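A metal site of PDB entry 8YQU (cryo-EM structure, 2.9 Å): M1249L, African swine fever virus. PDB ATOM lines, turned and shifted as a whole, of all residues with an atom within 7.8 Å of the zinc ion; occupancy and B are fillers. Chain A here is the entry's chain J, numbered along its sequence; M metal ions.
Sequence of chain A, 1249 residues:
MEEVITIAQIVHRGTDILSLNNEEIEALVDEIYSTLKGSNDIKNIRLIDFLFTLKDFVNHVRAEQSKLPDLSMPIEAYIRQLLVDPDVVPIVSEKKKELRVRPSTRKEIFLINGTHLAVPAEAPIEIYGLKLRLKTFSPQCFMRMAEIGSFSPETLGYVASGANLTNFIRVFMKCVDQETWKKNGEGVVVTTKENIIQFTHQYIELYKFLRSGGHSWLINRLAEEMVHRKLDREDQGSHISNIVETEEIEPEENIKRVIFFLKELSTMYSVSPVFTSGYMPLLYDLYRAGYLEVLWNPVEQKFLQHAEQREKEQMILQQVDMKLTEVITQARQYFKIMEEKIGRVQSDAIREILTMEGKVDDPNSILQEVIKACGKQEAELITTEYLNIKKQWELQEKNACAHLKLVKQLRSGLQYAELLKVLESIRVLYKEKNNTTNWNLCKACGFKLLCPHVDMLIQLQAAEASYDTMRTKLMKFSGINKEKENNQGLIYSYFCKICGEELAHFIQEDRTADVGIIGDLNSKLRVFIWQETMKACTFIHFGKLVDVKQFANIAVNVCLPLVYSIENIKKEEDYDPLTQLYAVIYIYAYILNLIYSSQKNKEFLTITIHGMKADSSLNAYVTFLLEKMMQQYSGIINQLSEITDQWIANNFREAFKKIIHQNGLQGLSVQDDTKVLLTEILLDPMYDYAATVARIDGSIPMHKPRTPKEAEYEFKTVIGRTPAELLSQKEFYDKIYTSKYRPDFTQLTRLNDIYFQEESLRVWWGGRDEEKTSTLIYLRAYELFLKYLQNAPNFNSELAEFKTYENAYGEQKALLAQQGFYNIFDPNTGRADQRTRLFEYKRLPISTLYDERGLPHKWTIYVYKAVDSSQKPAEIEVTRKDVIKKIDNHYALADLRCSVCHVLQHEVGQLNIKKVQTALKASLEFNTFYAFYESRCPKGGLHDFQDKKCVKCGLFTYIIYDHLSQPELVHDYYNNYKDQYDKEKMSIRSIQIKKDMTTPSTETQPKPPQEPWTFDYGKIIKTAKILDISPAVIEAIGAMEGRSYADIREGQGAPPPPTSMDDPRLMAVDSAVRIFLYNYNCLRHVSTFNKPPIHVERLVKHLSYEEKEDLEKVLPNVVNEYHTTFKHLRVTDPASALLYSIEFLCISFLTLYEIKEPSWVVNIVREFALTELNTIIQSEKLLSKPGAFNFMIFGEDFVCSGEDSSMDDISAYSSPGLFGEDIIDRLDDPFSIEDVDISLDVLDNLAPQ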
ATOM      1  N   SER A 847     -15.017  -1.839   4.722  1.00  0.00           N
ATOM      2  CA  SER A 847     -14.714  -2.597   3.523  1.00  0.00           C
ATOM      3  C   SER A 847     -13.285  -3.101   3.477  1.00  0.00           C
ATOM      4  O   SER A 847     -12.998  -4.044   2.739  1.00  0.00           O
ATOM      5  CB  SER A 847     -15.003  -1.747   2.286  1.00  0.00           C
ATOM      6  OG  SER A 847     -14.202  -0.578   2.277  1.00  0.00           O
ATOM      7  N   THR A 848     -12.378  -2.501   4.259  1.00  0.00           N
ATOM      8  CA  THR A 848     -10.992  -2.949   4.298  1.00  0.00           C
ATOM      9  C   THR A 848     -10.818  -4.280   5.022  1.00  0.00           C
ATOM     10  O   THR A 848      -9.856  -4.994   4.735  1.00  0.00           O
ATOM     11  CB  THR A 848     -10.114  -1.893   4.970  1.00  0.00           C
ATOM     12  OG1 THR A 848     -10.510  -1.753   6.351  1.00  0.00           O
ATOM     13  CG2 THR A 848     -10.278  -0.554   4.275  1.00  0.00           C
ATOM     14  N   LEU A 849     -11.726  -4.623   5.939  1.00  0.00           N
ATOM     15  CA  LEU A 849     -11.624  -5.863   6.693  1.00  0.00           C
ATOM     16  C   LEU A 849     -12.563  -6.956   6.204  1.00  0.00           C
ATOM     17  O   LEU A 849     -12.257  -8.139   6.343  1.00  0.00           O
ATOM     18  CB  LEU A 849     -11.886  -5.611   8.181  1.00  0.00           C
ATOM     19  CG  LEU A 849     -10.830  -4.832   8.956  1.00  0.00           C
ATOM     20  CD1 LEU A 849     -11.259  -4.650  10.404  1.00  0.00           C
ATOM     21  CD2 LEU A 849      -9.480  -5.537   8.879  1.00  0.00           C
ATOM     22  N   TYR A 850     -13.714  -6.584   5.634  1.00  0.00           N
ATOM     23  CA  TYR A 850     -14.709  -7.549   5.190  1.00  0.00           C
ATOM     24  C   TYR A 850     -15.204  -7.168   3.805  1.00  0.00           C
ATOM     25  O   TYR A 850     -15.231  -5.996   3.438  1.00  0.00           O
ATOM     26  CB  TYR A 850     -15.888  -7.617   6.176  1.00  0.00           C
ATOM     27  CG  TYR A 850     -15.476  -7.936   7.596  1.00  0.00           C
ATOM     28  CD1 TYR A 850     -15.277  -9.246   7.998  1.00  0.00           C
ATOM     29  CD2 TYR A 850     -15.273  -6.927   8.522  1.00  0.00           C
ATOM     30  CE1 TYR A 850     -14.887  -9.535   9.293  1.00  0.00           C
ATOM     31  CE2 TYR A 850     -14.891  -7.206   9.820  1.00  0.00           C
ATOM     32  CZ  TYR A 850     -14.703  -8.523  10.194  1.00  0.00           C
ATOM     33  OH  TYR A 850     -14.320  -8.805  11.479  1.00  0.00           O
ATOM     34  N   ASP A 851     -15.600  -8.182   3.041  1.00  0.00           N
ATOM     35  CA  ASP A 851     -16.059  -7.970   1.667  1.00  0.00           C
ATOM     36  C   ASP A 851     -17.570  -7.744   1.670  1.00  0.00           C
ATOM     37  O   ASP A 851     -18.201  -7.561   2.723  1.00  0.00           O
ATOM     38  CB  ASP A 851     -15.664  -9.152   0.783  1.00  0.00           C
ATOM     39  CG  ASP A 851     -16.293 -10.457   1.242  1.00  0.00           C
ATOM     40  OD1 ASP A 851     -16.581 -10.593   2.447  1.00  0.00           O
ATOM     41  OD2 ASP A 851     -16.491 -11.345   0.392  1.00  0.00           O
ATOM     42  N   GLU A 852     -18.176  -7.742   0.486  1.00  0.00           N
ATOM     43  CA  GLU A 852     -19.601  -7.485   0.353  1.00  0.00           C
ATOM     44  C   GLU A 852     -20.466  -8.645   0.841  1.00  0.00           C
ATOM     45  O   GLU A 852     -21.689  -8.482   0.920  1.00  0.00           O
ATOM     46  CB  GLU A 852     -19.944  -7.168  -1.110  1.00  0.00           C
ATOM     47  CG  GLU A 852     -19.514  -5.778  -1.551  1.00  0.00           C
ATOM     48  CD  GLU A 852     -19.724  -5.543  -3.032  1.00  0.00           C
ATOM     49  OE1 GLU A 852     -19.947  -6.529  -3.761  1.00  0.00           O
ATOM     50  OE2 GLU A 852     -19.673  -4.377  -3.462  1.00  0.00           O
ATOM     51  N   LEU A 855     -17.495 -11.793   4.714  1.00  0.00           N
ATOM     52  CA  LEU A 855     -16.367 -12.625   5.090  1.00  0.00           C
ATOM     53  C   LEU A 855     -15.096 -11.784   5.265  1.00  0.00           C
ATOM     54  O   LEU A 855     -14.944 -10.753   4.607  1.00  0.00           O
ATOM     55  CB  LEU A 855     -16.122 -13.705   4.042  1.00  0.00           C
ATOM     56  CG  LEU A 855     -17.217 -14.767   3.900  1.00  0.00           C
ATOM     57  CD1 LEU A 855     -16.946 -15.655   2.689  1.00  0.00           C
ATOM     58  CD2 LEU A 855     -17.327 -15.592   5.166  1.00  0.00           C
ATOM     59  N   PRO A 856     -14.198 -12.184   6.147  1.00  0.00           N
ATOM     60  CA  PRO A 856     -12.942 -11.441   6.312  1.00  0.00           C
ATOM     61  C   PRO A 856     -12.035 -11.608   5.106  1.00  0.00           C
ATOM     62  O   PRO A 856     -12.087 -12.589   4.366  1.00  0.00           O
ATOM     63  CB  PRO A 856     -12.318 -12.066   7.561  1.00  0.00           C
ATOM     64  CG  PRO A 856     -12.883 -13.434   7.626  1.00  0.00           C
ATOM     65  CD  PRO A 856     -14.278 -13.334   7.065  1.00  0.00           C
ATOM     66  N   HIS A 857     -11.182 -10.601   4.905  1.00  0.00           N
ATOM     67  CA  HIS A 857     -10.209 -10.641   3.817  1.00  0.00           C
ATOM     68  C   HIS A 857      -8.991 -11.470   4.210  1.00  0.00           C
ATOM     69  O   HIS A 857      -8.544 -11.426   5.351  1.00  0.00           O
ATOM     70  CB  HIS A 857      -9.772  -9.227   3.429  1.00  0.00           C
ATOM     71  CG  HIS A 857     -10.805  -8.467   2.650  1.00  0.00           C
ATOM     72  ND1 HIS A 857     -11.302  -8.911   1.451  1.00  0.00           N
ATOM     73  CD2 HIS A 857     -11.411  -7.278   2.904  1.00  0.00           C
ATOM     74  CE1 HIS A 857     -12.192  -8.040   0.999  1.00  0.00           C
ATOM     75  NE2 HIS A 857     -12.269  -7.034   1.864  1.00  0.00           N
ATOM     76  N   LYS A 858      -8.465 -12.223   3.240  1.00  0.00           N
ATOM     77  CA  LYS A 858      -7.240 -13.008   3.413  1.00  0.00           C
ATOM     78  C   LYS A 858      -6.320 -12.648   2.254  1.00  0.00           C
ATOM     79  O   LYS A 858      -6.352 -13.305   1.206  1.00  0.00           O
ATOM     80  CB  LYS A 858      -7.545 -14.496   3.461  1.00  0.00           C
ATOM     81  CG  LYS A 858      -8.345 -14.943   4.682  1.00  0.00           C
ATOM     82  CD  LYS A 858      -8.393 -16.453   4.779  1.00  0.00           C
ATOM     83  CE  LYS A 858      -9.185 -16.901   5.994  1.00  0.00           C
ATOM     84  NZ  LYS A 858     -10.633 -16.619   5.846  1.00  0.00           N
ATOM     85  N   TRP A 859      -5.498 -11.616   2.444  1.00  0.00           N
ATOM     86  CA  TRP A 859      -4.608 -11.150   1.397  1.00  0.00           C
ATOM     87  C   TRP A 859      -3.451 -12.124   1.232  1.00  0.00           C
ATOM     88  O   TRP A 859      -2.418 -11.981   1.895  1.00  0.00           O
ATOM     89  CB  TRP A 859      -4.087  -9.752   1.707  1.00  0.00           C
ATOM     90  CG  TRP A 859      -5.167  -8.771   2.046  1.00  0.00           C
ATOM     91  CD1 TRP A 859      -5.448  -8.260   3.279  1.00  0.00           C
ATOM     92  CD2 TRP A 859      -6.108  -8.195   1.143  1.00  0.00           C
ATOM     93  NE1 TRP A 859      -6.505  -7.395   3.195  1.00  0.00           N
ATOM     94  CE2 TRP A 859      -6.930  -7.328   1.894  1.00  0.00           C
ATOM     95  CE3 TRP A 859      -6.338  -8.310  -0.235  1.00  0.00           C
ATOM     96  CZ2 TRP A 859      -7.962  -6.602   1.326  1.00  0.00           C
ATOM     97  CZ3 TRP A 859      -7.365  -7.581  -0.795  1.00  0.00           C
ATOM     98  CH2 TRP A 859      -8.171  -6.739  -0.023  1.00  0.00           C
ATOM     99  N   ARG A 897      -3.749  -9.729  -3.291  1.00  0.00           N
ATOM    100  CA  ARG A 897      -5.085 -10.164  -3.649  1.00  0.00           C
ATOM    101  C   ARG A 897      -5.656 -11.071  -2.563  1.00  0.00           C
ATOM    102  O   ARG A 897      -4.930 -11.877  -1.970  1.00  0.00           O
ATOM    103  CB  ARG A 897      -5.102 -10.892  -5.007  1.00  0.00           C
ATOM    104  CG  ARG A 897      -6.488 -11.149  -5.555  1.00  0.00           C
ATOM    105  CD  ARG A 897      -6.429 -11.704  -6.964  1.00  0.00           C
ATOM    106  NE  ARG A 897      -6.047 -10.690  -7.942  1.00  0.00           N
ATOM    107  CZ  ARG A 897      -6.905  -9.924  -8.600  1.00  0.00           C
ATOM    108  NH1 ARG A 897      -8.210 -10.033  -8.406  1.00  0.00           N
ATOM    109  NH2 ARG A 897      -6.446  -9.028  -9.455  1.00  0.00           N
ATOM    110  N   CYS A 898      -6.951 -10.916  -2.302  1.00  0.00           N
ATOM    111  CA  CYS A 898      -7.651 -11.741  -1.337  1.00  0.00           C
ATOM    112  C   CYS A 898      -7.987 -13.089  -1.964  1.00  0.00           C
ATOM    113  O   CYS A 898      -8.466 -13.154  -3.097  1.00  0.00           O
ATOM    114  CB  CYS A 898      -8.921 -11.048  -0.855  1.00  0.00           C
ATOM    115  SG  CYS A 898      -9.819 -11.935   0.429  1.00  0.00           S
ATOM    116  N   SER A 899      -7.739 -14.170  -1.220  1.00  0.00           N
ATOM    117  CA  SER A 899      -8.025 -15.523  -1.672  1.00  0.00           C
ATOM    118  C   SER A 899      -9.460 -15.949  -1.403  1.00  0.00           C
ATOM    119  O   SER A 899      -9.760 -17.146  -1.439  1.00  0.00           O
ATOM    120  CB  SER A 899      -7.052 -16.506  -1.026  1.00  0.00           C
ATOM    121  OG  SER A 899      -7.239 -16.555   0.376  1.00  0.00           O
ATOM    122  N   VAL A 900     -10.358 -14.996  -1.138  1.00  0.00           N
ATOM    123  CA  VAL A 900     -11.758 -15.314  -0.866  1.00  0.00           C
ATOM    124  C   VAL A 900     -12.639 -14.579  -1.869  1.00  0.00           C
ATOM    125  O   VAL A 900     -13.363 -15.209  -2.646  1.00  0.00           O
ATOM    126  CB  VAL A 900     -12.138 -14.952   0.578  1.00  0.00           C
ATOM    127  CG1 VAL A 900     -13.627 -15.149   0.791  1.00  0.00           C
ATOM    128  CG2 VAL A 900     -11.343 -15.783   1.563  1.00  0.00           C
ATOM    129  N   CYS A 901     -12.584 -13.250  -1.861  1.00  0.00           N
ATOM    130  CA  CYS A 901     -13.406 -12.441  -2.750  1.00  0.00           C
ATOM    131  C   CYS A 901     -12.687 -12.048  -4.034  1.00  0.00           C
ATOM    132  O   CYS A 901     -13.332 -11.491  -4.936  1.00  0.00           O
ATOM    133  CB  CYS A 901     -13.877 -11.178  -2.016  1.00  0.00           C
ATOM    134  SG  CYS A 901     -12.543 -10.172  -1.331  1.00  0.00           S
ATOM    135  N   HIS A 902     -11.385 -12.310  -4.133  1.00  0.00           N
ATOM    136  CA  HIS A 902     -10.599 -12.046  -5.338  1.00  0.00           C
ATOM    137  C   HIS A 902     -10.682 -10.573  -5.755  1.00  0.00           C
ATOM    138  O   HIS A 902     -11.163 -10.223  -6.833  1.00  0.00           O
ATOM    139  CB  HIS A 902     -11.030 -12.968  -6.491  1.00  0.00           C
ATOM    140  CG  HIS A 902     -10.904 -14.421  -6.182  1.00  0.00           C
ATOM    141  ND1 HIS A 902     -11.966 -15.188  -5.737  1.00  0.00           N
ATOM    142  CD2 HIS A 902      -9.839 -15.255  -6.235  1.00  0.00           C
ATOM    143  CE1 HIS A 902     -11.557 -16.430  -5.544  1.00  0.00           C
ATOM    144  NE2 HIS A 902     -10.270 -16.501  -5.839  1.00  0.00           N
ATOM    145  N   VAL A 903     -10.206  -9.716  -4.860  1.00  0.00           N
ATOM    146  CA  VAL A 903     -10.142  -8.279  -5.106  1.00  0.00           C
ATOM    147  C   VAL A 903      -8.747  -7.789  -4.761  1.00  0.00           C
ATOM    148  O   VAL A 903      -8.090  -8.325  -3.863  1.00  0.00           O
ATOM    149  CB  VAL A 903     -11.214  -7.501  -4.307  1.00  0.00           C
ATOM    150  CG1 VAL A 903     -10.856  -7.442  -2.829  1.00  0.00           C
ATOM    151  CG2 VAL A 903     -11.404  -6.103  -4.866  1.00  0.00           C
ATOM    152  N   LEU A 911     -15.685  -1.431  -3.191  1.00  0.00           N
ATOM    153  CA  LEU A 911     -16.760  -2.177  -2.556  1.00  0.00           C
ATOM    154  C   LEU A 911     -17.776  -1.208  -1.944  1.00  0.00           C
ATOM    155  O   LEU A 911     -17.413  -0.153  -1.432  1.00  0.00           O
ATOM    156  CB  LEU A 911     -16.217  -3.107  -1.476  1.00  0.00           C
ATOM    157  CG  LEU A 911     -15.300  -4.238  -1.940  1.00  0.00           C
ATOM    158  CD1 LEU A 911     -14.715  -4.972  -0.745  1.00  0.00           C
ATOM    159  CD2 LEU A 911     -16.041  -5.199  -2.850  1.00  0.00           C
HETATM  160 ZN    ZN M   1     -11.911 -11.005   0.714  1.00  0.00          ZN
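The zinc ion is bound by SG of Cys 901 (2.3 Å). ND1 of His 857 binds the zinc ion. The zinc ion is bound by SG of Cys 898.
Merely in contact with the zinc ion: Val 900 and Pro 856. Five residues have an atom within 4 Å of the zinc ion: Pro 856, His 857, Cys 898, Val 900 and Cys 901. Along chain A the residues within 4 Å of the zinc ion span positions 856 to 901. The nearest printed residue that does not touch the zinc ion is Asp 851 (4.2 Å).
The backbone NH of His 857 is in hydrogen-bond range of the backbone carbonyl oxygen of Leu 849 (3.0 Å). The backbone carbonyl oxygen of Ser 847 is in hydrogen-bond range of a ring nitrogen (NE2) of His 857, at 3.2 Å. SG of Cys 898 sits close to N of Val 900 (3.5 Å). N of Lys 858 sits close to SG of Cys 898, 3.1 Å away. N of Cys 898 sits at hydrogen-bond distance from O of Val 903 (3.2 Å). A ring nitrogen (ND1) of His 902 sits at hydrogen-bond distance from the backbone carbonyl oxygen of Val 900 (3.4 Å).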
